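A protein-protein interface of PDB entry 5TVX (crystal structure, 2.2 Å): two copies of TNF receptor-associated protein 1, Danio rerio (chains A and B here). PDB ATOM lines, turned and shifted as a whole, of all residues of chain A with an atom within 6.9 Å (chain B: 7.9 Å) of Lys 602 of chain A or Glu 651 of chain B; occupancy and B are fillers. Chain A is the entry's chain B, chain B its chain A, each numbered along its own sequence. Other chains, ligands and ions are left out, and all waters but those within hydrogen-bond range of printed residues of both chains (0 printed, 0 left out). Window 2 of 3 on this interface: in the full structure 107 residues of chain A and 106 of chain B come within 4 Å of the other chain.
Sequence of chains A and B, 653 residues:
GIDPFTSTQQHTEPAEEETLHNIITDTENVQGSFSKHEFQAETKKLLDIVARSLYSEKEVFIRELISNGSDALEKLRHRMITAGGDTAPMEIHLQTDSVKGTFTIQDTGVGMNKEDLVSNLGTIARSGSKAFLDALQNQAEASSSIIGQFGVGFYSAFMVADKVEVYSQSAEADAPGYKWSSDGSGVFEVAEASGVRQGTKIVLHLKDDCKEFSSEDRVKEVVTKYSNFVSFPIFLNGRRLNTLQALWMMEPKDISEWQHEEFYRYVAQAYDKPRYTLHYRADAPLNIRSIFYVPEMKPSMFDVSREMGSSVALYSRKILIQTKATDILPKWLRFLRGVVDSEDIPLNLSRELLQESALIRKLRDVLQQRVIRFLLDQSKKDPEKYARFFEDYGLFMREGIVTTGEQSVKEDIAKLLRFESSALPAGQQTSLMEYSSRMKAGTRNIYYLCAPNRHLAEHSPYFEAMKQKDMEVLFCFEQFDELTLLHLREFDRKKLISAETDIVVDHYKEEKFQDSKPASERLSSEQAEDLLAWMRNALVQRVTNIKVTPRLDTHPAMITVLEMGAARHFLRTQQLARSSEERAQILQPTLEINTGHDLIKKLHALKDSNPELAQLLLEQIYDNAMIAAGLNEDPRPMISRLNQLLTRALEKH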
ATOM      1  N   LEU A 523     -23.982  25.531   2.631  1.00  0.00           N
ATOM      2  CA  LEU A 523     -24.168  24.915   1.327  1.00  0.00           C
ATOM      3  C   LEU A 523     -24.922  25.869   0.409  1.00  0.00           C
ATOM      4  O   LEU A 523     -25.767  26.648   0.847  1.00  0.00           O
ATOM      5  CB  LEU A 523     -24.938  23.597   1.449  1.00  0.00           C
ATOM      6  CG  LEU A 523     -24.404  22.503   2.374  1.00  0.00           C
ATOM      7  CD1 LEU A 523     -25.334  21.288   2.376  1.00  0.00           C
ATOM      8  CD2 LEU A 523     -22.997  22.097   1.970  1.00  0.00           C
ATOM      9  N   HIS A 597     -23.800  23.739   9.267  1.00  0.00           N
ATOM     10  CA  HIS A 597     -23.127  22.880  10.234  1.00  0.00           C
ATOM     11  C   HIS A 597     -22.171  21.929   9.528  1.00  0.00           C
ATOM     12  O   HIS A 597     -22.498  21.370   8.477  1.00  0.00           O
ATOM     13  CB  HIS A 597     -24.143  22.088  11.050  1.00  0.00           C
ATOM     14  CG  HIS A 597     -23.575  21.483  12.298  1.00  0.00           C
ATOM     15  ND1 HIS A 597     -22.805  20.340  12.289  1.00  0.00           N
ATOM     16  CD2 HIS A 597     -23.671  21.861  13.594  1.00  0.00           C
ATOM     17  CE1 HIS A 597     -22.452  20.038  13.525  1.00  0.00           C
ATOM     18  NE2 HIS A 597     -22.962  20.947  14.336  1.00  0.00           N
ATOM     19  N   ASP A 598     -20.983  21.741  10.121  1.00  0.00           N
ATOM     20  CA  ASP A 598     -19.956  20.918   9.477  1.00  0.00           C
ATOM     21  C   ASP A 598     -20.411  19.476   9.300  1.00  0.00           C
ATOM     22  O   ASP A 598     -19.972  18.801   8.369  1.00  0.00           O
ATOM     23  CB  ASP A 598     -18.652  20.952  10.277  1.00  0.00           C
ATOM     24  CG  ASP A 598     -18.013  22.335  10.309  1.00  0.00           C
ATOM     25  OD1 ASP A 598     -17.385  22.676  11.331  1.00  0.00           O
ATOM     26  OD2 ASP A 598     -18.139  23.081   9.315  1.00  0.00           O
ATOM     27  N   LEU A 599     -21.297  18.993  10.170  1.00  0.00           N
ATOM     28  CA  LEU A 599     -21.797  17.629  10.030  1.00  0.00           C
ATOM     29  C   LEU A 599     -22.723  17.503   8.826  1.00  0.00           C
ATOM     30  O   LEU A 599     -22.626  16.541   8.058  1.00  0.00           O
ATOM     31  CB  LEU A 599     -22.517  17.215  11.308  1.00  0.00           C
ATOM     32  CG  LEU A 599     -22.910  15.752  11.360  1.00  0.00           C
ATOM     33  CD1 LEU A 599     -21.671  14.902  11.142  1.00  0.00           C
ATOM     34  CD2 LEU A 599     -23.556  15.456  12.696  1.00  0.00           C
ATOM     35  N   ILE A 600     -23.626  18.469   8.647  1.00  0.00           N
ATOM     36  CA  ILE A 600     -24.483  18.486   7.470  1.00  0.00           C
ATOM     37  C   ILE A 600     -23.665  18.665   6.199  1.00  0.00           C
ATOM     38  O   ILE A 600     -23.916  17.997   5.188  1.00  0.00           O
ATOM     39  CB  ILE A 600     -25.539  19.590   7.602  1.00  0.00           C
ATOM     40  CG1 ILE A 600     -26.369  19.358   8.862  1.00  0.00           C
ATOM     41  CG2 ILE A 600     -26.405  19.626   6.348  1.00  0.00           C
ATOM     42  CD1 ILE A 600     -26.879  17.926   8.975  1.00  0.00           C
ATOM     43  N   LYS A 601     -22.700  19.591   6.213  1.00  0.00           N
ATOM     44  CA  LYS A 601     -21.882  19.788   5.023  1.00  0.00           C
ATOM     45  C   LYS A 601     -21.102  18.531   4.701  1.00  0.00           C
ATOM     46  O   LYS A 601     -20.914  18.199   3.525  1.00  0.00           O
ATOM     47  CB  LYS A 601     -20.945  20.987   5.204  1.00  0.00           C
ATOM     48  CG  LYS A 601     -21.688  22.294   5.492  1.00  0.00           C
ATOM     49  CD  LYS A 601     -20.845  23.543   5.230  1.00  0.00           C
ATOM     50  CE  LYS A 601     -19.760  23.734   6.272  1.00  0.00           C
ATOM     51  NZ  LYS A 601     -19.087  25.048   6.116  1.00  0.00           N
ATOM     52  N   LYS A 602     -20.677  17.794   5.726  1.00  0.00           N
ATOM     53  CA  LYS A 602     -19.988  16.538   5.461  1.00  0.00           C
ATOM     54  C   LYS A 602     -20.956  15.481   4.947  1.00  0.00           C
ATOM     55  O   LYS A 602     -20.609  14.700   4.054  1.00  0.00           O
ATOM     56  CB  LYS A 602     -19.274  16.046   6.716  1.00  0.00           C
ATOM     57  CG  LYS A 602     -18.603  14.690   6.535  1.00  0.00           C
ATOM     58  CD  LYS A 602     -17.622  14.705   5.379  1.00  0.00           C
ATOM     59  CE  LYS A 602     -16.371  15.513   5.710  1.00  0.00           C
ATOM     60  NZ  LYS A 602     -15.390  14.729   6.512  1.00  0.00           N
ATOM     61  N   LEU A 603     -22.172  15.433   5.498  1.00  0.00           N
ATOM     62  CA  LEU A 603     -23.158  14.483   4.995  1.00  0.00           C
ATOM     63  C   LEU A 603     -23.387  14.687   3.500  1.00  0.00           C
ATOM     64  O   LEU A 603     -23.434  13.717   2.730  1.00  0.00           O
ATOM     65  CB  LEU A 603     -24.468  14.618   5.779  1.00  0.00           C
ATOM     66  CG  LEU A 603     -25.632  13.728   5.333  1.00  0.00           C
ATOM     67  CD1 LEU A 603     -25.316  12.244   5.530  1.00  0.00           C
ATOM     68  CD2 LEU A 603     -26.917  14.125   6.066  1.00  0.00           C
ATOM     69  N   HIS A 604     -23.490  15.951   3.075  1.00  0.00           N
ATOM     70  CA  HIS A 604     -23.645  16.271   1.661  1.00  0.00           C
ATOM     71  C   HIS A 604     -22.483  15.744   0.824  1.00  0.00           C
ATOM     72  O   HIS A 604     -22.674  15.378  -0.340  1.00  0.00           O
ATOM     73  CB  HIS A 604     -23.780  17.783   1.483  1.00  0.00           C
ATOM     74  CG  HIS A 604     -23.486  18.254   0.093  1.00  0.00           C
ATOM     75  ND1 HIS A 604     -24.349  18.045  -0.963  1.00  0.00           N
ATOM     76  CD2 HIS A 604     -22.417  18.906  -0.420  1.00  0.00           C
ATOM     77  CE1 HIS A 604     -23.828  18.555  -2.063  1.00  0.00           C
ATOM     78  NE2 HIS A 604     -22.657  19.086  -1.760  1.00  0.00           N
ATOM     79  N   ALA A 605     -21.277  15.702   1.384  1.00  0.00           N
ATOM     80  CA  ALA A 605     -20.157  15.122   0.651  1.00  0.00           C
ATOM     81  C   ALA A 605     -20.191  13.600   0.694  1.00  0.00           C
ATOM     82  O   ALA A 605     -19.932  12.942  -0.321  1.00  0.00           O
ATOM     83  CB  ALA A 605     -18.829  15.635   1.207  1.00  0.00           C
ATOM     84  N   LEU A 606     -20.529  13.027   1.853  1.00  0.00           N
ATOM     85  CA  LEU A 606     -20.536  11.575   1.992  1.00  0.00           C
ATOM     86  C   LEU A 606     -21.525  10.902   1.047  1.00  0.00           C
ATOM     87  O   LEU A 606     -21.262   9.792   0.570  1.00  0.00           O
ATOM     88  CB  LEU A 606     -20.847  11.195   3.430  1.00  0.00           C
ATOM     89  CG  LEU A 606     -19.608  11.079   4.297  1.00  0.00           C
ATOM     90  CD1 LEU A 606     -19.993  10.571   5.665  1.00  0.00           C
ATOM     91  CD2 LEU A 606     -18.620  10.136   3.622  1.00  0.00           C
ATOM     92  N   LYS A 607     -22.651  11.556   0.747  1.00  0.00           N
ATOM     93  CA  LYS A 607     -23.679  10.912  -0.068  1.00  0.00           C
ATOM     94  C   LYS A 607     -23.152  10.517  -1.441  1.00  0.00           C
ATOM     95  O   LYS A 607     -23.667   9.575  -2.055  1.00  0.00           O
ATOM     96  CB  LYS A 607     -24.903  11.824  -0.208  1.00  0.00           C
ATOM     97  CG  LYS A 607     -24.702  13.028  -1.118  1.00  0.00           C
ATOM     98  CD  LYS A 607     -26.015  13.752  -1.383  1.00  0.00           C
ATOM     99  CE  LYS A 607     -25.810  14.985  -2.254  1.00  0.00           C
ATOM    100  NZ  LYS A 607     -25.315  14.650  -3.622  1.00  0.00           N
ATOM    101  N   SER A 609     -19.407  10.448  -1.941  1.00  0.00           N
ATOM    102  CA  SER A 609     -18.101   9.815  -1.754  1.00  0.00           C
ATOM    103  C   SER A 609     -18.215   8.446  -1.092  1.00  0.00           C
ATOM    104  O   SER A 609     -17.367   7.582  -1.314  1.00  0.00           O
ATOM    105  CB  SER A 609     -17.175  10.723  -0.938  1.00  0.00           C
ATOM    106  OG  SER A 609     -17.284  10.477   0.451  1.00  0.00           O
ATOM    107  N   ALA A 614     -22.904   7.584   4.319  1.00  0.00           N
ATOM    108  CA  ALA A 614     -23.809   8.722   4.462  1.00  0.00           C
ATOM    109  C   ALA A 614     -25.160   8.289   5.009  1.00  0.00           C
ATOM    110  O   ALA A 614     -25.758   8.986   5.842  1.00  0.00           O
ATOM    111  CB  ALA A 614     -23.990   9.430   3.121  1.00  0.00           C
ATOM    112  N   LEU A 617     -24.983   7.646   8.586  1.00  0.00           N
ATOM    113  CA  LEU A 617     -24.848   8.928   9.271  1.00  0.00           C
ATOM    114  C   LEU A 617     -26.173   9.677   9.301  1.00  0.00           C
ATOM    115  O   LEU A 617     -26.561  10.228  10.339  1.00  0.00           O
ATOM    116  CB  LEU A 617     -23.772   9.781   8.599  1.00  0.00           C
ATOM    117  CG  LEU A 617     -23.807  11.274   8.956  1.00  0.00           C
ATOM    118  CD1 LEU A 617     -23.531  11.503  10.449  1.00  0.00           C
ATOM    119  CD2 LEU A 617     -22.799  12.026   8.105  1.00  0.00           C
ATOM    120  N   ALA A 649     -16.837   5.163  10.810  1.00  0.00           N
ATOM    121  CA  ALA A 649     -16.350   6.536  10.731  1.00  0.00           C
ATOM    122  C   ALA A 649     -14.873   6.610  11.085  1.00  0.00           C
ATOM    123  O   ALA A 649     -14.092   7.279  10.397  1.00  0.00           O
ATOM    124  CB  ALA A 649     -17.162   7.440  11.654  1.00  0.00           C
ATOM    125  N   GLU A 651     -12.660   4.531  10.653  1.00  0.00           N
ATOM    126  CA  GLU A 651     -11.912   3.649   9.750  1.00  0.00           C
ATOM    127  C   GLU A 651     -11.678   2.275  10.366  1.00  0.00           C
ATOM    128  O   GLU A 651     -10.886   1.484   9.852  1.00  0.00           O
ATOM    129  CB  GLU A 651     -10.574   4.282   9.351  1.00  0.00           C
ATOM    130  CG  GLU A 651     -10.703   5.692   8.814  1.00  0.00           C
ATOM    131  CD  GLU A 651      -9.527   6.565   9.186  1.00  0.00           C
ATOM    132  OE1 GLU A 651      -9.246   7.518   8.433  1.00  0.00           O
ATOM    133  OE2 GLU A 651      -8.884   6.301  10.226  1.00  0.00           O
ATOM    134  N   ASN B 610      -4.858  10.846  18.856  1.00  0.00           N
ATOM    135  CA  ASN B 610      -5.742  12.000  18.969  1.00  0.00           C
ATOM    136  C   ASN B 610      -6.380  11.944  20.348  1.00  0.00           C
ATOM    137  O   ASN B 610      -7.468  11.373  20.512  1.00  0.00           O
ATOM    138  CB  ASN B 610      -6.802  12.000  17.865  1.00  0.00           C
ATOM    139  CG  ASN B 610      -7.509  13.337  17.736  1.00  0.00           C
ATOM    140  OD1 ASN B 610      -7.906  13.944  18.732  1.00  0.00           O
ATOM    141  ND2 ASN B 610      -7.667  13.806  16.503  1.00  0.00           N
ATOM    142  N   LEU B 613      -9.953  13.333  20.575  1.00  0.00           N
ATOM    143  CA  LEU B 613     -10.890  12.384  19.985  1.00  0.00           C
ATOM    144  C   LEU B 613     -11.043  11.150  20.867  1.00  0.00           C
ATOM    145  O   LEU B 613     -12.139  10.583  20.973  1.00  0.00           O
ATOM    146  CB  LEU B 613     -10.431  11.999  18.576  1.00  0.00           C
ATOM    147  CG  LEU B 613     -11.443  11.337  17.621  1.00  0.00           C
ATOM    148  CD1 LEU B 613     -11.524   9.825  17.821  1.00  0.00           C
ATOM    149  CD2 LEU B 613     -12.845  11.959  17.740  1.00  0.00           C
ATOM    150  N   LEU B 645     -18.155  14.336  18.534  1.00  0.00           N
ATOM    151  CA  LEU B 645     -17.448  13.097  18.221  1.00  0.00           C
ATOM    152  C   LEU B 645     -17.669  12.673  16.771  1.00  0.00           C
ATOM    153  O   LEU B 645     -16.711  12.359  16.050  1.00  0.00           O
ATOM    154  CB  LEU B 645     -17.896  11.992  19.182  1.00  0.00           C
ATOM    155  CG  LEU B 645     -17.568  10.546  18.796  1.00  0.00           C
ATOM    156  CD1 LEU B 645     -16.093  10.380  18.527  1.00  0.00           C
ATOM    157  CD2 LEU B 645     -17.991   9.596  19.891  1.00  0.00           C
ATOM    158  N   LEU B 646     -18.930  12.654  16.327  1.00  0.00           N
ATOM    159  CA  LEU B 646     -19.211  12.267  14.945  1.00  0.00           C
ATOM    160  C   LEU B 646     -18.543  13.217  13.958  1.00  0.00           C
ATOM    161  O   LEU B 646     -17.957  12.776  12.963  1.00  0.00           O
ATOM    162  CB  LEU B 646     -20.717  12.228  14.693  1.00  0.00           C
ATOM    163  CG  LEU B 646     -21.565  11.202  15.443  1.00  0.00           C
ATOM    164  CD1 LEU B 646     -23.027  11.527  15.237  1.00  0.00           C
ATOM    165  CD2 LEU B 646     -21.258   9.780  14.995  1.00  0.00           C
ATOM    166  N   THR B 647     -18.630  14.529  14.220  1.00  0.00           N
ATOM    167  CA  THR B 647     -18.042  15.521  13.326  1.00  0.00           C
ATOM    168  C   THR B 647     -16.521  15.427  13.293  1.00  0.00           C
ATOM    169  O   THR B 647     -15.906  15.698  12.256  1.00  0.00           O
ATOM    170  CB  THR B 647     -18.474  16.930  13.741  1.00  0.00           C
ATOM    171  OG1 THR B 647     -19.903  17.012  13.742  1.00  0.00           O
ATOM    172  CG2 THR B 647     -17.923  17.966  12.771  1.00  0.00           C
ATOM    173  N   ARG B 648     -15.896  15.043  14.406  1.00  0.00           N
ATOM    174  CA  ARG B 648     -14.446  14.921  14.415  1.00  0.00           C
ATOM    175  C   ARG B 648     -13.984  13.585  13.838  1.00  0.00           C
ATOM    176  O   ARG B 648     -12.936  13.525  13.186  1.00  0.00           O
ATOM    177  CB  ARG B 648     -13.926  15.116  15.841  1.00  0.00           C
ATOM    178  CG  ARG B 648     -12.426  14.949  15.994  1.00  0.00           C
ATOM    179  CD  ARG B 648     -11.637  16.089  15.377  1.00  0.00           C
ATOM    180  NE  ARG B 648     -10.284  16.133  15.925  1.00  0.00           N
ATOM    181  CZ  ARG B 648      -9.982  16.644  17.115  1.00  0.00           C
ATOM    182  NH1 ARG B 648     -10.940  17.159  17.882  1.00  0.00           N
ATOM    183  NH2 ARG B 648      -8.721  16.640  17.537  1.00  0.00           N
ATOM    184  N   ALA B 649     -14.761  12.517  14.037  1.00  0.00           N
ATOM    185  CA  ALA B 649     -14.421  11.219  13.465  1.00  0.00           C
ATOM    186  C   ALA B 649     -14.451  11.226  11.940  1.00  0.00           C
ATOM    187  O   ALA B 649     -13.753  10.418  11.315  1.00  0.00           O
ATOM    188  CB  ALA B 649     -15.376  10.146  13.988  1.00  0.00           C
ATOM    189  N   LEU B 650     -15.239  12.117  11.333  1.00  0.00           N
ATOM    190  CA  LEU B 650     -15.438  12.161   9.885  1.00  0.00           C
ATOM    191  C   LEU B 650     -14.595  13.289   9.299  1.00  0.00           C
ATOM    192  O   LEU B 650     -15.007  14.450   9.306  1.00  0.00           O
ATOM    193  CB  LEU B 650     -16.916  12.354   9.563  1.00  0.00           C
ATOM    194  CG  LEU B 650     -17.854  11.228  10.005  1.00  0.00           C
ATOM    195  CD1 LEU B 650     -19.285  11.722  10.060  1.00  0.00           C
ATOM    196  CD2 LEU B 650     -17.730  10.019   9.086  1.00  0.00           C
ATOM    197  N   GLU B 651     -13.418  12.948   8.787  1.00  0.00           N
ATOM    198  CA  GLU B 651     -12.540  13.927   8.146  1.00  0.00           C
ATOM    199  C   GLU B 651     -11.793  13.289   6.985  1.00  0.00           C
ATOM    200  O   GLU B 651     -11.098  12.287   7.158  1.00  0.00           O
ATOM    201  CB  GLU B 651     -11.550  14.511   9.155  1.00  0.00           C
ATOM    202  CG  GLU B 651     -12.167  15.493  10.137  1.00  0.00           C
ATOM    203  CD  GLU B 651     -11.289  15.726  11.354  1.00  0.00           C
ATOM    204  OE1 GLU B 651     -10.633  14.762  11.805  1.00  0.00           O
ATOM    205  OE2 GLU B 651     -11.255  16.871  11.858  1.00  0.00           O
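The side-chain amino group (NZ) of Lys 602 of chain A lies within hydrogen-bond range of the backbone carbonyl oxygen (O) of Leu 650 of chain B, 2.8 Å away.
The side-chain amino group (NZ) of Lys 602 of chain A lies close to the backbone NH (N) of Glu 651 of chain B (3.5 Å).
The backbone carbonyl oxygen (O) of Ala 649 of chain B lies close to the backbone carbonyl oxygen (O) of Ala 649 of chain A, 3.3 Å away.
ND1 of His 597 of chain A sits at hydrogen-bond distance from N of Leu 599 of chain A (2.9 Å).
The side-chain amino group (NZ) of Lys 601 of chain A lies within salt-bridge range of the side-chain carboxylate (OD2) of Asp 598 of chain A (3.9 Å).
Among the printed residues, pairs that only touch across the chains: Leu 599 of chain A with Thr 647 of chain B (3.6 Å), Ala 649 of chain A with Leu 650 of chain B (3.7 Å), Asp 598 of chain A with Thr 647 of chain B (3.96 Å) and His 597 of chain A with Thr 647 of chain B (3.96 Å).
Printed residues of chain B within 4 Å of Asp 598 of chain A: Thr 647.
Of the printed residues of chain B, Leu 599 of chain A touches Thr 647 (3.6 Å).
Of chain B, only Leu 650 and Glu 651 come within 4 Å of Lys 602 of chain A.
Of the printed residues of chain A, Ala 649 of chain B touches Ala 649.
Of the 9 printed residues of chain B, 4 touch a printed residue of chain A.
Printed residues of chain B that touch a printed residue of chain A: Thr 647, Ala 649, Leu 650 and Glu 651.
Hydrophobic or aromatic side chains of chain B within 4 Å of the printed part of chain A: Ala 649 and Leu 650.
Of the 17 printed residues of chain A, 5 touch a printed residue of chain B.
Printed residues of chain A that touch a printed residue of chain B: His 597, Asp 598, Leu 599, Lys 602 and Ala 649.
Among the printed residues, 7 pairs touch across the chains.
Among the printed residues, no Asp or Glu carboxylate lies within 4 Å of a Lys or Arg side-chain nitrogen of the other chain.
Ala 649 of chain B touches its own counterpart, Ala 649 of chain A.
Positions printed for both chains: 649 and 651.
Of the 7 pairs that touch across the chains among the printed residues, 1 has its exchanged pair printed and touching as well.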
